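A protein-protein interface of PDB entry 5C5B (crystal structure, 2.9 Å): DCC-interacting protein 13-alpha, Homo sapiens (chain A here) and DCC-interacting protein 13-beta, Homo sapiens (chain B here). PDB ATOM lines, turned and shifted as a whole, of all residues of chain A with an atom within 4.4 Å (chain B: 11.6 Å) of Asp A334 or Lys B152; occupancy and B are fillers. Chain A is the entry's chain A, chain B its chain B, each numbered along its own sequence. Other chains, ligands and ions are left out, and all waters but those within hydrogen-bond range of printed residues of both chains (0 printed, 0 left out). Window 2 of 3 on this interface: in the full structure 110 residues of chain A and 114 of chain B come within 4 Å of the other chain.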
ATOM      1  N   VAL A 333     -18.350  15.863 -28.424  1.00  0.00           N
ATOM      2  CA  VAL A 333     -17.616  15.493 -27.223  1.00  0.00           C
ATOM      3  C   VAL A 333     -18.525  15.585 -26.003  1.00  0.00           C
ATOM      4  O   VAL A 333     -19.362  16.482 -25.913  1.00  0.00           O
ATOM      5  CB  VAL A 333     -16.369  16.401 -27.037  1.00  0.00           C
ATOM      6  CG1 VAL A 333     -15.825  16.325 -25.618  1.00  0.00           C
ATOM      7  CG2 VAL A 333     -15.288  16.031 -28.043  1.00  0.00           C
ATOM      8  N   ASP A 334     -18.369  14.650 -25.070  1.00  0.00           N
ATOM      9  CA  ASP A 334     -19.072  14.738 -23.800  1.00  0.00           C
ATOM     10  C   ASP A 334     -18.177  15.405 -22.765  1.00  0.00           C
ATOM     11  O   ASP A 334     -17.090  14.910 -22.464  1.00  0.00           O
ATOM     12  CB  ASP A 334     -19.485  13.348 -23.310  1.00  0.00           C
ATOM     13  CG  ASP A 334     -20.626  12.760 -24.113  1.00  0.00           C
ATOM     14  OD1 ASP A 334     -21.631  13.467 -24.325  1.00  0.00           O
ATOM     15  OD2 ASP A 334     -20.518  11.586 -24.527  1.00  0.00           O
ATOM     16  N   CYS A 335     -18.627  16.533 -22.230  1.00  0.00           N
ATOM     17  CA  CYS A 335     -17.867  17.226 -21.198  1.00  0.00           C
ATOM     18  C   CYS A 335     -18.782  17.882 -20.170  1.00  0.00           C
ATOM     19  O   CYS A 335     -19.700  18.620 -20.532  1.00  0.00           O
ATOM     20  CB  CYS A 335     -16.951  18.275 -21.832  1.00  0.00           C
ATOM     21  SG  CYS A 335     -16.154  19.384 -20.653  1.00  0.00           S
ATOM     22  N   ASP A 337     -21.203  17.067 -18.484  1.00  0.00           N
ATOM     23  CA  ASP A 337     -22.626  16.756 -18.642  1.00  0.00           C
ATOM     24  C   ASP A 337     -23.359  17.811 -19.485  1.00  0.00           C
ATOM     25  O   ASP A 337     -24.582  17.943 -19.415  1.00  0.00           O
ATOM     26  CB  ASP A 337     -23.292  16.610 -17.265  1.00  0.00           C
ATOM     27  CG  ASP A 337     -24.643  15.915 -17.330  1.00  0.00           C
ATOM     28  OD1 ASP A 337     -25.021  15.435 -18.419  1.00  0.00           O
ATOM     29  OD2 ASP A 337     -25.326  15.850 -16.287  1.00  0.00           O
ATOM     30  N   ARG A 338     -22.602  18.579 -20.261  1.00  0.00           N
ATOM     31  CA  ARG A 338     -23.168  19.690 -21.023  1.00  0.00           C
ATOM     32  C   ARG A 338     -23.743  19.212 -22.355  1.00  0.00           C
ATOM     33  O   ARG A 338     -23.313  18.193 -22.894  1.00  0.00           O
ATOM     34  CB  ARG A 338     -22.135  20.791 -21.256  1.00  0.00           C
ATOM     35  CG  ARG A 338     -21.611  21.432 -19.984  1.00  0.00           C
ATOM     36  CD  ARG A 338     -21.665  22.948 -20.104  1.00  0.00           C
ATOM     37  NE  ARG A 338     -21.316  23.628 -18.861  1.00  0.00           N
ATOM     38  CZ  ARG A 338     -21.512  24.924 -18.640  1.00  0.00           C
ATOM     39  NH1 ARG A 338     -22.062  25.681 -19.580  1.00  0.00           N
ATOM     40  NH2 ARG A 338     -21.162  25.463 -17.481  1.00  0.00           N
ATOM     41  N   ARG A 339     -24.716  19.950 -22.879  1.00  0.00           N
ATOM     42  CA  ARG A 339     -25.362  19.586 -24.135  1.00  0.00           C
ATOM     43  C   ARG A 339     -24.721  20.243 -25.346  1.00  0.00           C
ATOM     44  O   ARG A 339     -24.351  21.413 -25.296  1.00  0.00           O
ATOM     45  CB  ARG A 339     -26.839  19.963 -24.123  1.00  0.00           C
ATOM     46  CG  ARG A 339     -27.673  19.128 -23.206  1.00  0.00           C
ATOM     47  CD  ARG A 339     -29.138  19.402 -23.423  1.00  0.00           C
ATOM     48  NE  ARG A 339     -29.449  20.742 -23.897  1.00  0.00           N
ATOM     49  CZ  ARG A 339     -30.486  21.009 -24.686  1.00  0.00           C
ATOM     50  NH1 ARG A 339     -30.726  22.251 -25.083  1.00  0.00           N
ATOM     51  NH2 ARG A 339     -31.283  20.025 -25.079  1.00  0.00           N
ATOM     52  N   LYS B 146     -28.356  29.590 -17.663  1.00  0.00           N
ATOM     53  CA  LYS B 146     -29.016  28.483 -16.984  1.00  0.00           C
ATOM     54  C   LYS B 146     -29.569  27.468 -17.990  1.00  0.00           C
ATOM     55  O   LYS B 146     -29.862  26.323 -17.641  1.00  0.00           O
ATOM     56  CB  LYS B 146     -30.138  29.007 -16.081  1.00  0.00           C
ATOM     57  CG  LYS B 146     -31.532  28.730 -16.643  1.00  0.00           C
ATOM     58  CD  LYS B 146     -32.614  28.786 -15.584  1.00  0.00           C
ATOM     59  CE  LYS B 146     -32.739  30.176 -14.996  1.00  0.00           C
ATOM     60  NZ  LYS B 146     -33.693  30.208 -13.853  1.00  0.00           N
ATOM     61  N   TYR B 147     -29.691  27.888 -19.244  1.00  0.00           N
ATOM     62  CA  TYR B 147     -29.963  26.957 -20.330  1.00  0.00           C
ATOM     63  C   TYR B 147     -28.721  26.127 -20.649  1.00  0.00           C
ATOM     64  O   TYR B 147     -28.792  24.904 -20.776  1.00  0.00           O
ATOM     65  CB  TYR B 147     -30.435  27.716 -21.566  1.00  0.00           C
ATOM     66  CG  TYR B 147     -30.889  26.833 -22.700  1.00  0.00           C
ATOM     67  CD1 TYR B 147     -29.999  26.402 -23.673  1.00  0.00           C
ATOM     68  CD2 TYR B 147     -32.214  26.430 -22.794  1.00  0.00           C
ATOM     69  CE1 TYR B 147     -30.418  25.597 -24.710  1.00  0.00           C
ATOM     70  CE2 TYR B 147     -32.641  25.625 -23.825  1.00  0.00           C
ATOM     71  CZ  TYR B 147     -31.739  25.212 -24.780  1.00  0.00           C
ATOM     72  OH  TYR B 147     -32.160  24.408 -25.809  1.00  0.00           O
ATOM     73  N   SER B 148     -27.592  26.812 -20.801  1.00  0.00           N
ATOM     74  CA  SER B 148     -26.302  26.166 -21.021  1.00  0.00           C
ATOM     75  C   SER B 148     -26.008  25.093 -19.978  1.00  0.00           C
ATOM     76  O   SER B 148     -25.530  24.011 -20.318  1.00  0.00           O
ATOM     77  CB  SER B 148     -25.175  27.203 -21.031  1.00  0.00           C
ATOM     78  OG  SER B 148     -25.040  27.829 -19.769  1.00  0.00           O
ATOM     79  N   ARG B 149     -26.286  25.389 -18.710  1.00  0.00           N
ATOM     80  CA  ARG B 149     -25.931  24.446 -17.644  1.00  0.00           C
ATOM     81  C   ARG B 149     -26.808  23.186 -17.559  1.00  0.00           C
ATOM     82  O   ARG B 149     -26.520  22.295 -16.760  1.00  0.00           O
ATOM     83  CB  ARG B 149     -25.929  25.149 -16.286  1.00  0.00           C
ATOM     84  CG  ARG B 149     -24.806  26.159 -16.124  1.00  0.00           C
ATOM     85  CD  ARG B 149     -24.663  26.592 -14.677  1.00  0.00           C
ATOM     86  NE  ARG B 149     -25.868  27.252 -14.186  1.00  0.00           N
ATOM     87  CZ  ARG B 149     -26.113  28.550 -14.321  1.00  0.00           C
ATOM     88  NH1 ARG B 149     -27.238  29.067 -13.845  1.00  0.00           N
ATOM     89  NH2 ARG B 149     -25.232  29.333 -14.929  1.00  0.00           N
ATOM     90  N   LEU B 150     -27.866  23.113 -18.362  1.00  0.00           N
ATOM     91  CA  LEU B 150     -28.762  21.951 -18.356  1.00  0.00           C
ATOM     92  C   LEU B 150     -28.005  20.644 -18.621  1.00  0.00           C
ATOM     93  O   LEU B 150     -27.042  20.628 -19.387  1.00  0.00           O
ATOM     94  CB  LEU B 150     -29.874  22.130 -19.396  1.00  0.00           C
ATOM     95  CG  LEU B 150     -30.932  23.203 -19.128  1.00  0.00           C
ATOM     96  CD1 LEU B 150     -31.992  23.188 -20.220  1.00  0.00           C
ATOM     97  CD2 LEU B 150     -31.568  23.019 -17.758  1.00  0.00           C
ATOM     98  N   PRO B 151     -28.446  19.537 -17.993  1.00  0.00           N
ATOM     99  CA  PRO B 151     -27.703  18.276 -18.077  1.00  0.00           C
ATOM    100  C   PRO B 151     -27.934  17.531 -19.390  1.00  0.00           C
ATOM    101  O   PRO B 151     -29.016  17.611 -19.965  1.00  0.00           O
ATOM    102  CB  PRO B 151     -28.240  17.473 -16.885  1.00  0.00           C
ATOM    103  CG  PRO B 151     -29.567  18.111 -16.522  1.00  0.00           C
ATOM    104  CD  PRO B 151     -29.762  19.346 -17.358  1.00  0.00           C
ATOM    105  N   LYS B 152     -26.900  16.846 -19.870  1.00  0.00           N
ATOM    106  CA  LYS B 152     -26.986  16.053 -21.094  1.00  0.00           C
ATOM    107  C   LYS B 152     -27.449  14.614 -20.861  1.00  0.00           C
ATOM    108  O   LYS B 152     -28.451  14.177 -21.427  1.00  0.00           O
ATOM    109  CB  LYS B 152     -25.637  16.040 -21.814  1.00  0.00           C
ATOM    110  CG  LYS B 152     -25.681  15.396 -23.191  1.00  0.00           C
ATOM    111  CD  LYS B 152     -24.285  15.203 -23.762  1.00  0.00           C
ATOM    112  CE  LYS B 152     -24.336  14.876 -25.248  1.00  0.00           C
ATOM    113  NZ  LYS B 152     -25.192  13.692 -25.527  1.00  0.00           N
ATOM    114  N   LYS B 153     -26.706  13.885 -20.028  1.00  0.00           N
ATOM    115  CA  LYS B 153     -26.920  12.451 -19.848  1.00  0.00           C
ATOM    116  C   LYS B 153     -28.275  12.137 -19.219  1.00  0.00           C
ATOM    117  O   LYS B 153     -29.045  11.347 -19.764  1.00  0.00           O
ATOM    118  CB  LYS B 153     -25.803  11.854 -18.989  1.00  0.00           C
ATOM    119  N   LYS B 154     -28.567  12.748 -18.075  1.00  0.00           N
ATOM    120  CA  LYS B 154     -29.854  12.536 -17.424  1.00  0.00           C
ATOM    121  C   LYS B 154     -30.717  13.772 -17.629  1.00  0.00           C
ATOM    122  O   LYS B 154     -30.463  14.826 -17.049  1.00  0.00           O
ATOM    123  CB  LYS B 154     -29.675  12.241 -15.935  1.00  0.00           C
ATOM    124  N   GLU B 155     -31.732  13.642 -18.472  1.00  0.00           N
ATOM    125  CA  GLU B 155     -32.523  14.797 -18.860  1.00  0.00           C
ATOM    126  C   GLU B 155     -33.970  14.840 -18.402  1.00  0.00           C
ATOM    127  O   GLU B 155     -34.791  14.012 -18.801  1.00  0.00           O
ATOM    128  CB  GLU B 155     -32.492  14.944 -20.375  1.00  0.00           C
ATOM    129  CG  GLU B 155     -31.563  16.043 -20.801  1.00  0.00           C
ATOM    130  CD  GLU B 155     -31.486  16.206 -22.295  1.00  0.00           C
ATOM    131  OE1 GLU B 155     -31.985  15.333 -23.034  1.00  0.00           O
ATOM    132  OE2 GLU B 155     -30.930  17.224 -22.730  1.00  0.00           O
ATOM    133  N   ASN B 156     -34.276  15.849 -17.596  1.00  0.00           N
ATOM    134  CA  ASN B 156     -35.654  16.185 -17.282  1.00  0.00           C
ATOM    135  C   ASN B 156     -36.184  17.101 -18.373  1.00  0.00           C
ATOM    136  O   ASN B 156     -35.771  18.256 -18.488  1.00  0.00           O
ATOM    137  CB  ASN B 156     -35.772  16.852 -15.914  1.00  0.00           C
ATOM    138  CG  ASN B 156     -37.163  16.734 -15.327  1.00  0.00           C
ATOM    139  OD1 ASN B 156     -38.151  16.657 -16.056  1.00  0.00           O
ATOM    140  ND2 ASN B 156     -37.248  16.709 -14.002  1.00  0.00           N
ATOM    141  N   GLU B 157     -37.071  16.572 -19.203  1.00  0.00           N
ATOM    142  CA  GLU B 157     -37.556  17.307 -20.363  1.00  0.00           C
ATOM    143  C   GLU B 157     -38.386  18.514 -19.940  1.00  0.00           C
ATOM    144  O   GLU B 157     -38.402  19.531 -20.629  1.00  0.00           O
ATOM    145  CB  GLU B 157     -38.366  16.387 -21.278  1.00  0.00           C
ATOM    146  CG  GLU B 157     -37.514  15.731 -22.351  1.00  0.00           C
ATOM    147  CD  GLU B 157     -38.329  14.930 -23.342  1.00  0.00           C
ATOM    148  OE1 GLU B 157     -39.537  14.733 -23.092  1.00  0.00           O
ATOM    149  OE2 GLU B 157     -37.764  14.494 -24.368  1.00  0.00           O
ATOM    150  N   VAL B 159     -38.080  20.462 -17.002  1.00  0.00           N
ATOM    151  CA  VAL B 159     -37.147  21.514 -16.610  1.00  0.00           C
ATOM    152  C   VAL B 159     -36.492  22.107 -17.857  1.00  0.00           C
ATOM    153  O   VAL B 159     -36.390  23.324 -17.988  1.00  0.00           O
ATOM    154  CB  VAL B 159     -36.077  20.990 -15.602  1.00  0.00           C
ATOM    155  CG1 VAL B 159     -34.655  21.309 -16.051  1.00  0.00           C
ATOM    156  CG2 VAL B 159     -36.347  21.532 -14.201  1.00  0.00           C
ATOM    157  N   LYS B 160     -36.076  21.242 -18.778  1.00  0.00           N
ATOM    158  CA  LYS B 160     -35.413  21.677 -20.000  1.00  0.00           C
ATOM    159  C   LYS B 160     -36.318  22.539 -20.882  1.00  0.00           C
ATOM    160  O   LYS B 160     -35.901  23.593 -21.365  1.00  0.00           O
ATOM    161  CB  LYS B 160     -34.916  20.462 -20.783  1.00  0.00           C
ATOM    162  CG  LYS B 160     -34.757  20.696 -22.270  1.00  0.00           C
ATOM    163  CD  LYS B 160     -34.215  19.456 -22.947  1.00  0.00           C
ATOM    164  CE  LYS B 160     -34.540  19.459 -24.425  1.00  0.00           C
ATOM    165  NZ  LYS B 160     -36.007  19.349 -24.644  1.00  0.00           N
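O of Asp A337 touches O of Leu B150, 3.6 Å away. Asp A337 touches Pro B151. NH1 of Arg A338 touches OG of Ser B148, at 3.7 Å. Arg B149 touches Arg A338 (CG to NH2, 3.95 Å). O of Arg A338 touches CD of Lys B152, 3.3 Å away. Arg A339 touches Pro B151. Lys B152 touches Arg A339 (CA to CG, 3.8 Å). Lys B160 touches Arg A339 (CE to NH2, 3.4 Å).
Of chain B, only Lys B152 comes within 4 Å of Asp A334. Lys B152 touches just these residues of chain A: Asp A334, Asp A337, Arg A338 and Arg A339. No residue of chain B comes within 4 Å of Val A333. No residue of chain B comes within 4 Å of Cys A335. Of chain B, only Leu B150, Pro B151, Lys B152 and Lys B153 come within 4 Å of Asp A337. Of the printed residues of chain A, Lys B153 touches Asp A337. Of the printed residues of chain B, Arg A339 touches Tyr B147, Pro B151, Lys B152, Glu B155 and Lys B160. Glu B157 touches none of the printed residues of chain A. The nearest printed residue of chain B that does not touch Arg A339 is Leu B150 (4.2 Å).
OD1 of Asp A334 lies within salt-bridge range of NZ of Lys B152, at 3.8 Å. The backbone carbonyl oxygen (O) of Asp A337 lies within hydrogen-bond range of the backbone NH (N) of Lys B152 (2.6 Å). The backbone NH (N) of Lys B153 lies within hydrogen-bond range of the side-chain carboxylate (OD1) of Asp A337. The side-chain hydroxyl (OH) of Tyr B147 lies within hydrogen-bond range of the guanidinium group (NH1) of Arg A339 (2.7 Å). The side-chain carboxylate (OE2) of Glu B155 lies within salt-bridge range of the guanidinium group (NH2) of Arg A339 (3.7 Å).
Of the 6 printed residues of chain A, 4 touch a printed residue of chain B.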
